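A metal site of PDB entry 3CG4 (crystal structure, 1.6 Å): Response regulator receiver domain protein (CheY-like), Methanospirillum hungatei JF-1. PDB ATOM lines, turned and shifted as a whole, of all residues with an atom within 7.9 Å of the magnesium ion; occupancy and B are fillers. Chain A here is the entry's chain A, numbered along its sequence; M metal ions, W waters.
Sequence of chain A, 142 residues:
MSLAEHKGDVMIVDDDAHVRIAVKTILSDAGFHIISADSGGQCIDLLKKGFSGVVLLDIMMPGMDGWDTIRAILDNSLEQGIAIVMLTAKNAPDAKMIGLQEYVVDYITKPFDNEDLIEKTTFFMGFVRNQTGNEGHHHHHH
The magnesium ion is bound by OD2 of Asp 58 (2.2 Å).
The magnesium ion is bound by the backbone carbonyl oxygen (O) of Met 60.
The magnesium ion is bound by water W1, at 2.2 Å.
Water W2 is bound to the magnesium ion.
The magnesium ion is bound by OD1 of Asp 15 (2.3 Å).
The magnesium ion has five donor atoms within binding distance.
Water W1 lies within hydrogen-bond range of the side-chain carboxylate of Asp 14 and the side-chain amino group of Lys 110.
OD1 of Asp 58 is in salt-bridge range of NZ of Lys 110, 3.2 Å away.
N of Asp 58 is in hydrogen-bond range of O of Val 13, 2.9 Å away.
Within 4 Å of the magnesium ion: Asp 15, Asp 58 and Met 60.
The nearest printed residue that does not touch the magnesium ion is Asp 14 (4.03 Å).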
ATOM      1  N   VAL A  13      15.329  14.814 -13.830  1.00  0.00           N
ATOM      2  CA  VAL A  13      16.033  13.905 -12.948  1.00  0.00           C
ATOM      3  C   VAL A  13      15.085  12.774 -12.633  1.00  0.00           C
ATOM      4  O   VAL A  13      14.131  12.959 -11.887  1.00  0.00           O
ATOM      5  CB  VAL A  13      16.484  14.571 -11.609  1.00  0.00           C
ATOM      6  CG1 VAL A  13      17.414  13.647 -10.832  1.00  0.00           C
ATOM      7  CG2 VAL A  13      17.142  15.925 -11.862  1.00  0.00           C
ATOM      8  N   ASP A  14      15.348  11.610 -13.218  1.00  0.00           N
ATOM      9  CA  ASP A  14      14.460  10.475 -13.002  1.00  0.00           C
ATOM     10  C   ASP A  14      15.283   9.224 -13.227  1.00  0.00           C
ATOM     11  O   ASP A  14      16.045   9.202 -14.168  1.00  0.00           O
ATOM     12  CB  ASP A  14      13.277  10.542 -13.964  1.00  0.00           C
ATOM     13  CG  ASP A  14      12.130   9.644 -13.546  1.00  0.00           C
ATOM     14  OD1 ASP A  14      12.285   8.407 -13.534  1.00  0.00           O
ATOM     15  OD2 ASP A  14      11.067  10.191 -13.220  1.00  0.00           O
ATOM     16  N   ASP A  15      15.095   8.218 -12.375  1.00  0.00           N
ATOM     17  CA  ASP A  15      15.893   6.979 -12.517  1.00  0.00           C
ATOM     18  C   ASP A  15      15.467   6.156 -13.745  1.00  0.00           C
ATOM     19  O   ASP A  15      16.200   5.287 -14.225  1.00  0.00           O
ATOM     20  CB  ASP A  15      15.875   6.143 -11.226  1.00  0.00           C
ATOM     21  CG  ASP A  15      14.490   5.696 -10.843  1.00  0.00           C
ATOM     22  OD1 ASP A  15      13.636   6.561 -10.584  1.00  0.00           O
ATOM     23  OD2 ASP A  15      14.243   4.471 -10.782  1.00  0.00           O
ATOM     24  N   ASP A  16      14.271   6.451 -14.254  1.00  0.00           N
ATOM     25  CA  ASP A  16      13.719   5.716 -15.417  1.00  0.00           C
ATOM     26  C   ASP A  16      14.057   6.359 -16.762  1.00  0.00           C
ATOM     27  O   ASP A  16      13.593   7.454 -17.104  1.00  0.00           O
ATOM     28  CB  ASP A  16      12.216   5.573 -15.237  1.00  0.00           C
ATOM     29  CG  ASP A  16      11.613   4.474 -16.103  1.00  0.00           C
ATOM     30  OD1 ASP A  16      12.087   4.263 -17.238  1.00  0.00           O
ATOM     31  OD2 ASP A  16      10.645   3.841 -15.636  1.00  0.00           O
ATOM     32  N   VAL A  19      11.076   7.571 -18.864  1.00  0.00           N
ATOM     33  CA  VAL A  19      10.584   8.870 -18.418  1.00  0.00           C
ATOM     34  C   VAL A  19      11.475  10.005 -18.955  1.00  0.00           C
ATOM     35  O   VAL A  19      10.980  10.981 -19.497  1.00  0.00           O
ATOM     36  CB  VAL A  19      10.407   8.953 -16.889  1.00  0.00           C
ATOM     37  CG1 VAL A  19       9.936  10.350 -16.472  1.00  0.00           C
ATOM     38  CG2 VAL A  19       9.439   7.869 -16.406  1.00  0.00           C
ATOM     39  N   ASP A  58      12.263  13.586  -9.761  1.00  0.00           N
ATOM     40  CA  ASP A  58      11.564  12.361  -9.344  1.00  0.00           C
ATOM     41  C   ASP A  58      11.721  12.132  -7.820  1.00  0.00           C
ATOM     42  O   ASP A  58      12.841  12.104  -7.296  1.00  0.00           O
ATOM     43  CB  ASP A  58      12.197  11.207 -10.098  1.00  0.00           C
ATOM     44  CG  ASP A  58      11.423   9.950  -9.998  1.00  0.00           C
ATOM     45  OD1 ASP A  58      10.229   9.972  -9.612  1.00  0.00           O
ATOM     46  OD2 ASP A  58      12.014   8.907 -10.325  1.00  0.00           O
ATOM     47  N   ILE A  59      10.605  11.985  -7.091  1.00  0.00           N
ATOM     48  CA  ILE A  59      10.698  11.722  -5.661  1.00  0.00           C
ATOM     49  C   ILE A  59      11.223  10.328  -5.339  1.00  0.00           C
ATOM     50  O   ILE A  59      12.044  10.184  -4.445  1.00  0.00           O
ATOM     51  CB  ILE A  59       9.350  11.920  -4.900  1.00  0.00           C
ATOM     52  CG1 ILE A  59       8.826  13.336  -5.073  1.00  0.00           C
ATOM     53  CG2 ILE A  59       9.526  11.659  -3.402  1.00  0.00           C
ATOM     54  CD1 ILE A  59       7.807  13.754  -3.970  1.00  0.00           C
ATOM     55  N   MET A  60      10.720   9.320  -6.041  1.00  0.00           N
ATOM     56  CA  MET A  60      11.158   7.962  -5.722  1.00  0.00           C
ATOM     57  C   MET A  60      12.256   7.491  -6.658  1.00  0.00           C
ATOM     58  O   MET A  60      12.023   7.083  -7.800  1.00  0.00           O
ATOM     59  CB  MET A  60       9.999   6.951  -5.643  1.00  0.00           C
ATOM     60  CG  MET A  60      10.443   5.561  -5.109  1.00  0.00           C
ATOM     61  SD  MET A  60      11.760   5.587  -3.623  1.00  0.00           S
ATOM     62  CE  MET A  60      12.626   3.854  -3.959  1.00  0.00           C
ATOM     63  N   MET A  61      13.459   7.549  -6.123  1.00  0.00           N
ATOM     64  CA  MET A  61      14.637   7.064  -6.812  1.00  0.00           C
ATOM     65  C   MET A  61      15.371   6.166  -5.851  1.00  0.00           C
ATOM     66  O   MET A  61      15.363   6.408  -4.635  1.00  0.00           O
ATOM     67  CB  MET A  61      15.532   8.228  -7.240  1.00  0.00           C
ATOM     68  CG  MET A  61      14.884   9.099  -8.305  1.00  0.00           C
ATOM     69  SD  MET A  61      16.139  10.343  -9.083  1.00  0.00           S
ATOM     70  CE  MET A  61      16.374  11.499  -7.510  1.00  0.00           C
ATOM     71  N   PRO A  62      16.001   5.095  -6.372  1.00  0.00           N
ATOM     72  CA  PRO A  62      16.710   4.233  -5.423  1.00  0.00           C
ATOM     73  C   PRO A  62      17.991   4.850  -4.871  1.00  0.00           C
ATOM     74  O   PRO A  62      18.691   5.552  -5.583  1.00  0.00           O
ATOM     75  CB  PRO A  62      17.024   2.969  -6.241  1.00  0.00           C
ATOM     76  CG  PRO A  62      16.994   3.408  -7.658  1.00  0.00           C
ATOM     77  CD  PRO A  62      16.086   4.616  -7.752  1.00  0.00           C
ATOM     78  N   LEU A  87       8.238  15.257  -9.070  1.00  0.00           N
ATOM     79  CA  LEU A  87       7.383  14.273  -9.729  1.00  0.00           C
ATOM     80  C   LEU A  87       7.083  13.226  -8.685  1.00  0.00           C
ATOM     81  O   LEU A  87       7.982  12.537  -8.180  1.00  0.00           O
ATOM     82  CB  LEU A  87       8.071  13.623 -10.937  1.00  0.00           C
ATOM     83  CG  LEU A  87       8.871  14.498 -11.906  1.00  0.00           C
ATOM     84  CD1 LEU A  87       9.364  13.650 -13.053  1.00  0.00           C
ATOM     85  CD2 LEU A  87       8.054  15.658 -12.431  1.00  0.00           C
ATOM     86  N   LYS A 110       2.555  11.383 -11.084  1.00  0.00           N
ATOM     87  CA  LYS A 110       2.626  10.342 -12.102  1.00  0.00           C
ATOM     88  C   LYS A 110       1.446   9.380 -11.967  1.00  0.00           C
ATOM     89  O   LYS A 110       1.111   8.990 -10.855  1.00  0.00           O
ATOM     90  CB  LYS A 110       3.914   9.536 -11.959  1.00  0.00           C
ATOM     91  CG  LYS A 110       5.154  10.303 -12.385  1.00  0.00           C
ATOM     92  CD  LYS A 110       6.359   9.394 -12.122  1.00  0.00           C
ATOM     93  CE  LYS A 110       7.637   9.952 -12.709  1.00  0.00           C
ATOM     94  NZ  LYS A 110       8.775   9.064 -12.272  1.00  0.00           N
HETATM   95 MG    MG M   1      11.466   6.822  -9.915  1.00  0.00          MG
HETATM   96  O   HOH W   1      10.924   6.817 -12.093  1.00  0.00           O
HETATM   97  O   HOH W   2      11.460   4.597  -9.603  1.00  0.00           O
